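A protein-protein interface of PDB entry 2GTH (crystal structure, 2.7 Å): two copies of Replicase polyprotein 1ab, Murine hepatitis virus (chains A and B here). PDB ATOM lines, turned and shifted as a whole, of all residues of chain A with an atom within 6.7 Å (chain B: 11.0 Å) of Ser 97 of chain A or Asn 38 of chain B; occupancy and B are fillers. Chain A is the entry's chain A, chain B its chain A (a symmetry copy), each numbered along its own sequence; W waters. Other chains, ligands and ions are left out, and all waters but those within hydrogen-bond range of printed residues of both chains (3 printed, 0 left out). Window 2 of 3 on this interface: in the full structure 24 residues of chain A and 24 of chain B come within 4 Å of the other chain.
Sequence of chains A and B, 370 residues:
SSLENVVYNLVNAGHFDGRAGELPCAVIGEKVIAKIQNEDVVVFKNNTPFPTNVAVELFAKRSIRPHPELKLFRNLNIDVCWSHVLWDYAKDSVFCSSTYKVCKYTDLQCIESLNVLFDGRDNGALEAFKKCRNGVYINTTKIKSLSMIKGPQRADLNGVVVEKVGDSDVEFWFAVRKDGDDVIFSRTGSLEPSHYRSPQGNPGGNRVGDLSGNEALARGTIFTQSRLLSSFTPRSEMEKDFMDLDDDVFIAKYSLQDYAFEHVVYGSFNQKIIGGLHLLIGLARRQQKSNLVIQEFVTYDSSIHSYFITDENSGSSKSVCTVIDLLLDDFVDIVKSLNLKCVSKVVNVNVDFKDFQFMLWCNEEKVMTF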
ATOM      1  N   PRO A  49      24.280   3.376   0.151  1.00  0.00           N
ATOM      2  CA  PRO A  49      23.954   3.522  -1.265  1.00  0.00           C
ATOM      3  C   PRO A  49      25.192   3.402  -2.155  1.00  0.00           C
ATOM      4  O   PRO A  49      25.079   3.426  -3.381  1.00  0.00           O
ATOM      5  CB  PRO A  49      23.327   4.910  -1.320  1.00  0.00           C
ATOM      6  CG  PRO A  49      24.146   5.645  -0.328  1.00  0.00           C
ATOM      7  CD  PRO A  49      24.212   4.678   0.835  1.00  0.00           C
ATOM      8  N   PHE A  50      26.365   3.252  -1.537  1.00  0.00           N
ATOM      9  CA  PHE A  50      27.640   3.152  -2.281  1.00  0.00           C
ATOM     10  C   PHE A  50      27.983   1.746  -2.774  1.00  0.00           C
ATOM     11  O   PHE A  50      27.354   0.770  -2.381  1.00  0.00           O
ATOM     12  CB  PHE A  50      28.805   3.610  -1.393  1.00  0.00           C
ATOM     13  CG  PHE A  50      28.603   4.953  -0.746  1.00  0.00           C
ATOM     14  CD1 PHE A  50      28.914   6.124  -1.428  1.00  0.00           C
ATOM     15  CD2 PHE A  50      28.142   5.041   0.567  1.00  0.00           C
ATOM     16  CE1 PHE A  50      28.780   7.351  -0.821  1.00  0.00           C
ATOM     17  CE2 PHE A  50      28.005   6.272   1.184  1.00  0.00           C
ATOM     18  CZ  PHE A  50      28.328   7.433   0.487  1.00  0.00           C
ATOM     19  N   ASP A  79      26.113  19.469   5.564  1.00  0.00           N
ATOM     20  CA  ASP A  79      26.172  18.859   4.257  1.00  0.00           C
ATOM     21  C   ASP A  79      27.273  17.813   4.173  1.00  0.00           C
ATOM     22  O   ASP A  79      27.097  16.786   3.542  1.00  0.00           O
ATOM     23  CB  ASP A  79      26.356  19.942   3.188  1.00  0.00           C
ATOM     24  CG  ASP A  79      25.060  20.691   2.895  1.00  0.00           C
ATOM     25  OD1 ASP A  79      24.045  20.010   2.661  1.00  0.00           O
ATOM     26  OD2 ASP A  79      25.048  21.938   2.886  1.00  0.00           O
ATOM     27  N   VAL A  80      28.401  18.060   4.820  1.00  0.00           N
ATOM     28  CA  VAL A  80      29.508  17.112   4.775  1.00  0.00           C
ATOM     29  C   VAL A  80      30.446  17.312   5.970  1.00  0.00           C
ATOM     30  O   VAL A  80      30.446  18.378   6.597  1.00  0.00           O
ATOM     31  CB  VAL A  80      30.320  17.264   3.454  1.00  0.00           C
ATOM     32  CG1 VAL A  80      30.963  18.649   3.384  1.00  0.00           C
ATOM     33  CG2 VAL A  80      31.382  16.195   3.380  1.00  0.00           C
ATOM     34  N   LYS A  91      20.693   4.404  10.898  1.00  0.00           N
ATOM     35  CA  LYS A  91      20.569   4.313   9.468  1.00  0.00           C
ATOM     36  C   LYS A  91      21.316   3.095   8.913  1.00  0.00           C
ATOM     37  O   LYS A  91      21.025   2.605   7.825  1.00  0.00           O
ATOM     38  CB  LYS A  91      21.126   5.590   8.852  1.00  0.00           C
ATOM     39  CG  LYS A  91      20.751   5.770   7.423  1.00  0.00           C
ATOM     40  CD  LYS A  91      20.891   7.225   6.991  1.00  0.00           C
ATOM     41  CE  LYS A  91      22.327   7.571   6.709  1.00  0.00           C
ATOM     42  NZ  LYS A  91      22.409   8.751   5.850  1.00  0.00           N
ATOM     43  N   VAL A  94      26.427   5.549   6.268  1.00  0.00           N
ATOM     44  CA  VAL A  94      27.177   6.785   6.500  1.00  0.00           C
ATOM     45  C   VAL A  94      26.203   7.949   6.694  1.00  0.00           C
ATOM     46  O   VAL A  94      25.081   7.930   6.189  1.00  0.00           O
ATOM     47  CB  VAL A  94      28.120   7.110   5.313  1.00  0.00           C
ATOM     48  CG1 VAL A  94      28.591   8.546   5.397  1.00  0.00           C
ATOM     49  CG2 VAL A  94      29.320   6.198   5.336  1.00  0.00           C
ATOM     50  N   PHE A  95      26.623   8.958   7.438  1.00  0.00           N
ATOM     51  CA  PHE A  95      25.756  10.093   7.675  1.00  0.00           C
ATOM     52  C   PHE A  95      25.501  10.982   6.461  1.00  0.00           C
ATOM     53  O   PHE A  95      24.413  10.977   5.885  1.00  0.00           O
ATOM     54  CB  PHE A  95      26.299  10.936   8.830  1.00  0.00           C
ATOM     55  CG  PHE A  95      25.551  12.208   9.036  1.00  0.00           C
ATOM     56  CD1 PHE A  95      24.180  12.264   8.803  1.00  0.00           C
ATOM     57  CD2 PHE A  95      26.208  13.345   9.476  1.00  0.00           C
ATOM     58  CE1 PHE A  95      23.479  13.431   9.002  1.00  0.00           C
ATOM     59  CE2 PHE A  95      25.510  14.526   9.684  1.00  0.00           C
ATOM     60  CZ  PHE A  95      24.137  14.569   9.446  1.00  0.00           C
ATOM     61  N   CYS A  96      26.498  11.772   6.098  1.00  0.00           N
ATOM     62  CA  CYS A  96      26.355  12.648   4.957  1.00  0.00           C
ATOM     63  C   CYS A  96      26.521  11.762   3.754  1.00  0.00           C
ATOM     64  O   CYS A  96      27.177  10.721   3.843  1.00  0.00           O
ATOM     65  CB  CYS A  96      27.421  13.722   4.981  1.00  0.00           C
ATOM     66  SG  CYS A  96      27.228  14.790   6.375  1.00  0.00           S
ATOM     67  N   SER A  97      25.910  12.151   2.638  1.00  0.00           N
ATOM     68  CA  SER A  97      26.004  11.338   1.449  1.00  0.00           C
ATOM     69  C   SER A  97      27.295  11.652   0.720  1.00  0.00           C
ATOM     70  O   SER A  97      27.657  10.963  -0.236  1.00  0.00           O
ATOM     71  CB  SER A  97      24.795  11.560   0.547  1.00  0.00           C
ATOM     72  OG  SER A  97      24.686  12.910   0.176  1.00  0.00           O
ATOM     73  N   SER A  98      28.005  12.672   1.207  1.00  0.00           N
ATOM     74  CA  SER A  98      29.276  13.076   0.621  1.00  0.00           C
ATOM     75  C   SER A  98      30.434  12.990   1.605  1.00  0.00           C
ATOM     76  O   SER A  98      30.225  13.056   2.813  1.00  0.00           O
ATOM     77  CB  SER A  98      29.185  14.509   0.125  1.00  0.00           C
ATOM     78  OG  SER A  98      27.967  14.731  -0.542  1.00  0.00           O
ATOM     79  N   THR A  99      31.655  12.848   1.087  1.00  0.00           N
ATOM     80  CA  THR A  99      32.848  12.805   1.937  1.00  0.00           C
ATOM     81  C   THR A  99      33.857  13.863   1.480  1.00  0.00           C
ATOM     82  O   THR A  99      33.784  14.358   0.350  1.00  0.00           O
ATOM     83  CB  THR A  99      33.548  11.414   1.939  1.00  0.00           C
ATOM     84  OG1 THR A  99      33.957  11.078   0.607  1.00  0.00           O
ATOM     85  CG2 THR A  99      32.622  10.342   2.495  1.00  0.00           C
ATOM     86  N   THR A 106      34.820   8.818  -3.110  1.00  0.00           N
ATOM     87  CA  THR A 106      33.687   9.681  -2.831  1.00  0.00           C
ATOM     88  C   THR A 106      33.970  11.151  -2.460  1.00  0.00           C
ATOM     89  O   THR A 106      33.095  11.996  -2.588  1.00  0.00           O
ATOM     90  CB  THR A 106      32.816   9.042  -1.742  1.00  0.00           C
ATOM     91  OG1 THR A 106      33.611   8.778  -0.589  1.00  0.00           O
ATOM     92  CG2 THR A 106      32.245   7.751  -2.234  1.00  0.00           C
ATOM     93  N   LEU A 114      29.135  24.671   0.739  1.00  0.00           N
ATOM     94  CA  LEU A 114      28.406  23.679   1.532  1.00  0.00           C
ATOM     95  C   LEU A 114      28.501  24.004   3.013  1.00  0.00           C
ATOM     96  O   LEU A 114      29.385  24.750   3.425  1.00  0.00           O
ATOM     97  CB  LEU A 114      28.964  22.275   1.284  1.00  0.00           C
ATOM     98  CG  LEU A 114      28.766  21.667  -0.098  1.00  0.00           C
ATOM     99  CD1 LEU A 114      29.476  20.331  -0.200  1.00  0.00           C
ATOM    100  CD2 LEU A 114      27.289  21.501  -0.345  1.00  0.00           C
ATOM    101  N   LEU B  23       9.843  12.120  -4.685  1.00  0.00           N
ATOM    102  CA  LEU B  23      11.021  12.076  -3.827  1.00  0.00           C
ATOM    103  C   LEU B  23      12.101  11.402  -4.669  1.00  0.00           C
ATOM    104  O   LEU B  23      11.858  10.370  -5.297  1.00  0.00           O
ATOM    105  CB  LEU B  23      10.734  11.258  -2.567  1.00  0.00           C
ATOM    106  CG  LEU B  23      11.140  11.882  -1.247  1.00  0.00           C
ATOM    107  CD1 LEU B  23      10.686  13.292  -1.291  1.00  0.00           C
ATOM    108  CD2 LEU B  23      10.513  11.175  -0.051  1.00  0.00           C
ATOM    109  N   PRO B  24      13.297  11.984  -4.714  1.00  0.00           N
ATOM    110  CA  PRO B  24      14.360  11.371  -5.516  1.00  0.00           C
ATOM    111  C   PRO B  24      14.697   9.966  -5.021  1.00  0.00           C
ATOM    112  O   PRO B  24      14.803   9.741  -3.817  1.00  0.00           O
ATOM    113  CB  PRO B  24      15.525  12.349  -5.349  1.00  0.00           C
ATOM    114  CG  PRO B  24      14.832  13.672  -5.122  1.00  0.00           C
ATOM    115  CD  PRO B  24      13.717  13.292  -4.182  1.00  0.00           C
ATOM    116  N   CYS B  25      14.864   9.019  -5.940  1.00  0.00           N
ATOM    117  CA  CYS B  25      15.186   7.650  -5.526  1.00  0.00           C
ATOM    118  C   CYS B  25      16.311   6.988  -6.295  1.00  0.00           C
ATOM    119  O   CYS B  25      16.755   7.448  -7.345  1.00  0.00           O
ATOM    120  CB  CYS B  25      13.973   6.725  -5.659  1.00  0.00           C
ATOM    121  SG  CYS B  25      12.500   7.191  -4.786  1.00  0.00           S
ATOM    122  N   ALA B  26      16.740   5.865  -5.747  1.00  0.00           N
ATOM    123  CA  ALA B  26      17.766   5.043  -6.337  1.00  0.00           C
ATOM    124  C   ALA B  26      17.446   3.592  -5.956  1.00  0.00           C
ATOM    125  O   ALA B  26      17.215   3.253  -4.788  1.00  0.00           O
ATOM    126  CB  ALA B  26      19.117   5.436  -5.824  1.00  0.00           C
ATOM    127  N   ILE B  33      16.532   3.483  -2.044  1.00  0.00           N
ATOM    128  CA  ILE B  33      17.085   4.633  -1.342  1.00  0.00           C
ATOM    129  C   ILE B  33      16.380   5.936  -1.694  1.00  0.00           C
ATOM    130  O   ILE B  33      16.251   6.284  -2.864  1.00  0.00           O
ATOM    131  CB  ILE B  33      18.581   4.795  -1.681  1.00  0.00           C
ATOM    132  CG1 ILE B  33      19.406   3.749  -0.944  1.00  0.00           C
ATOM    133  CG2 ILE B  33      19.046   6.177  -1.331  1.00  0.00           C
ATOM    134  CD1 ILE B  33      19.247   2.364  -1.473  1.00  0.00           C
ATOM    135  N   ALA B  34      15.928   6.663  -0.681  1.00  0.00           N
ATOM    136  CA  ALA B  34      15.256   7.940  -0.917  1.00  0.00           C
ATOM    137  C   ALA B  34      16.182   9.075  -0.533  1.00  0.00           C
ATOM    138  O   ALA B  34      16.779   9.040   0.533  1.00  0.00           O
ATOM    139  CB  ALA B  34      13.985   8.025  -0.090  1.00  0.00           C
ATOM    140  N   LYS B  35      16.329  10.073  -1.396  1.00  0.00           N
ATOM    141  CA  LYS B  35      17.186  11.190  -1.027  1.00  0.00           C
ATOM    142  C   LYS B  35      16.271  12.122  -0.265  1.00  0.00           C
ATOM    143  O   LYS B  35      15.379  12.723  -0.830  1.00  0.00           O
ATOM    144  CB  LYS B  35      17.793  11.908  -2.247  1.00  0.00           C
ATOM    145  CG  LYS B  35      18.935  12.872  -1.842  1.00  0.00           C
ATOM    146  CD  LYS B  35      19.813  13.349  -3.023  1.00  0.00           C
ATOM    147  CE  LYS B  35      20.639  12.225  -3.689  1.00  0.00           C
ATOM    148  NZ  LYS B  35      21.775  11.704  -2.889  1.00  0.00           N
ATOM    149  N   ILE B  36      16.478  12.208   1.035  1.00  0.00           N
ATOM    150  CA  ILE B  36      15.659  13.056   1.864  1.00  0.00           C
ATOM    151  C   ILE B  36      16.525  14.056   2.619  1.00  0.00           C
ATOM    152  O   ILE B  36      17.439  13.666   3.361  1.00  0.00           O
ATOM    153  CB  ILE B  36      14.845  12.199   2.846  1.00  0.00           C
ATOM    154  CG1 ILE B  36      13.752  11.473   2.069  1.00  0.00           C
ATOM    155  CG2 ILE B  36      14.271  13.056   3.960  1.00  0.00           C
ATOM    156  CD1 ILE B  36      12.988  10.489   2.874  1.00  0.00           C
ATOM    157  N   GLN B  37      16.236  15.344   2.420  1.00  0.00           N
ATOM    158  CA  GLN B  37      16.997  16.397   3.076  1.00  0.00           C
ATOM    159  C   GLN B  37      18.458  16.274   2.662  1.00  0.00           C
ATOM    160  O   GLN B  37      19.368  16.465   3.475  1.00  0.00           O
ATOM    161  CB  GLN B  37      16.882  16.240   4.588  1.00  0.00           C
ATOM    162  CG  GLN B  37      16.221  17.405   5.280  1.00  0.00           C
ATOM    163  CD  GLN B  37      14.952  17.866   4.576  1.00  0.00           C
ATOM    164  OE1 GLN B  37      15.008  18.529   3.529  1.00  0.00           O
ATOM    165  NE2 GLN B  37      13.796  17.515   5.148  1.00  0.00           N
ATOM    166  N   ASN B  38      18.659  15.930   1.393  1.00  0.00           N
ATOM    167  CA  ASN B  38      19.986  15.759   0.820  1.00  0.00           C
ATOM    168  C   ASN B  38      20.782  14.579   1.366  1.00  0.00           C
ATOM    169  O   ASN B  38      21.930  14.368   0.985  1.00  0.00           O
ATOM    170  CB  ASN B  38      20.794  17.036   0.985  1.00  0.00           C
ATOM    171  CG  ASN B  38      21.140  17.645  -0.333  1.00  0.00           C
ATOM    172  OD1 ASN B  38      20.270  18.168  -1.036  1.00  0.00           O
ATOM    173  ND2 ASN B  38      22.411  17.559  -0.706  1.00  0.00           N
ATOM    174  N   GLU B  39      20.160  13.819   2.256  1.00  0.00           N
ATOM    175  CA  GLU B  39      20.780  12.642   2.872  1.00  0.00           C
ATOM    176  C   GLU B  39      20.083  11.390   2.325  1.00  0.00           C
ATOM    177  O   GLU B  39      18.858  11.319   2.336  1.00  0.00           O
ATOM    178  CB  GLU B  39      20.626  12.742   4.403  1.00  0.00           C
ATOM    179  CG  GLU B  39      20.826  11.459   5.192  1.00  0.00           C
ATOM    180  CD  GLU B  39      20.701  11.689   6.688  1.00  0.00           C
ATOM    181  OE1 GLU B  39      19.828  12.470   7.101  1.00  0.00           O
ATOM    182  OE2 GLU B  39      21.469  11.094   7.472  1.00  0.00           O
ATOM    183  N   ASP B  40      20.851  10.417   1.838  1.00  0.00           N
ATOM    184  CA  ASP B  40      20.261   9.190   1.290  1.00  0.00           C
ATOM    185  C   ASP B  40      19.829   8.220   2.383  1.00  0.00           C
ATOM    186  O   ASP B  40      20.579   7.942   3.316  1.00  0.00           O
ATOM    187  CB  ASP B  40      21.253   8.463   0.378  1.00  0.00           C
ATOM    188  CG  ASP B  40      21.780   9.339  -0.742  1.00  0.00           C
ATOM    189  OD1 ASP B  40      20.959   9.950  -1.473  1.00  0.00           O
ATOM    190  OD2 ASP B  40      23.026   9.406  -0.888  1.00  0.00           O
ATOM    191  N   VAL B  41      18.624   7.683   2.264  1.00  0.00           N
ATOM    192  CA  VAL B  41      18.141   6.744   3.269  1.00  0.00           C
ATOM    193  C   VAL B  41      17.378   5.569   2.634  1.00  0.00           C
ATOM    194  O   VAL B  41      16.645   5.728   1.660  1.00  0.00           O
ATOM    195  CB  VAL B  41      17.253   7.475   4.304  1.00  0.00           C
ATOM    196  CG1 VAL B  41      16.067   8.095   3.611  1.00  0.00           C
ATOM    197  CG2 VAL B  41      16.781   6.521   5.377  1.00  0.00           C
ATOM    198  N   VAL B  42      17.587   4.381   3.181  1.00  0.00           N
ATOM    199  CA  VAL B  42      16.919   3.195   2.686  1.00  0.00           C
ATOM    200  C   VAL B  42      15.563   3.160   3.355  1.00  0.00           C
ATOM    201  O   VAL B  42      15.473   3.150   4.581  1.00  0.00           O
ATOM    202  CB  VAL B  42      17.709   1.910   3.042  1.00  0.00           C
ATOM    203  CG1 VAL B  42      16.829   0.692   2.869  1.00  0.00           C
ATOM    204  CG2 VAL B  42      18.938   1.784   2.154  1.00  0.00           C
HETATM  205  O   HOH W   1      19.368   4.107   5.143  1.00  0.00           O
HETATM  206  O   HOH W   2      22.737  14.202  -1.595  1.00  0.00           O
HETATM  207  O   HOH W   3      24.141  14.111   2.956  1.00  0.00           O
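The backbone carbonyl oxygen (O) of Asn 38 of chain B is in hydrogen-bond range of the side-chain hydroxyl (OG) of Ser 97 of chain A (3.2 Å).
OE2 of Glu 39 of chain B sits close to O of Phe 95 of chain A (3.3 Å).
The side-chain amino group (NZ) of Lys 91 of chain A lies within salt-bridge range of the side-chain carboxylate (OE2) of Glu 39 of chain B (3.0 Å).
The side-chain amino group (NZ) of Lys 91 of chain A lies within hydrogen-bond range of the backbone carbonyl oxygen (O) of Asp 40 of chain B (3.2 Å).
The side-chain amino group (NZ) of Lys 91 of chain A lies within hydrogen-bond range of the backbone carbonyl oxygen (O) of Phe 95 of chain A.
The side-chain amino group (NZ) of Lys 35 of chain B lies within salt-bridge range of the side-chain carboxylate (OD2) of Asp 40 of chain B (3.3 Å).
The backbone carbonyl oxygen of Val 94 of chain A sits at hydrogen-bond distance from the side-chain amino group of Lys 91 of chain A.
Among the printed residues, pairs that only touch across the chains: Ser 97 of chain A with Asp 40 of chain B and Pro 49 of chain A with Asp 40 of chain B.
Printed residues of chain B within 4 Å of Lys 91 of chain A: Glu 39 (3.0 Å) and Asp 40 (3.2 Å).
No residue of chain B comes within 4 Å of Cys 96 of chain A.
Of chain B, only Asn 38 (3.2 Å) and Asp 40 (3.1 Å) come within 4 Å of Ser 97 of chain A.
No residue of chain B comes within 4 Å of Ser 98 of chain A.
Asn 38 of chain B touches just one residue of chain A: Ser 97.
Printed residues of chain A within 4 Å of Asp 40 of chain B: Pro 49 (3.96 Å), Lys 91 (3.2 Å) and Ser 97 (3.1 Å).
No position is printed for both chains.
Of the 6 pairs that touch across the chains among the printed residues, none has its exchanged pair printed and touching as well.
Water W3 lies within hydrogen-bond range of the backbone NH (N) of Ser 97 of chain A and the backbone carbonyl oxygen (O) of Asn 38 of chain B.
Water W1 lies within hydrogen-bond range of N of Val 42 of chain B and O of Lys 91 of chain A.
Water W2 lies within hydrogen-bond range of O of Asn 38 of chain B (2.7 Å), OG of Ser 97 of chain A (2.9 Å) and NZ of Lys 35 of chain B (3.0 Å).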
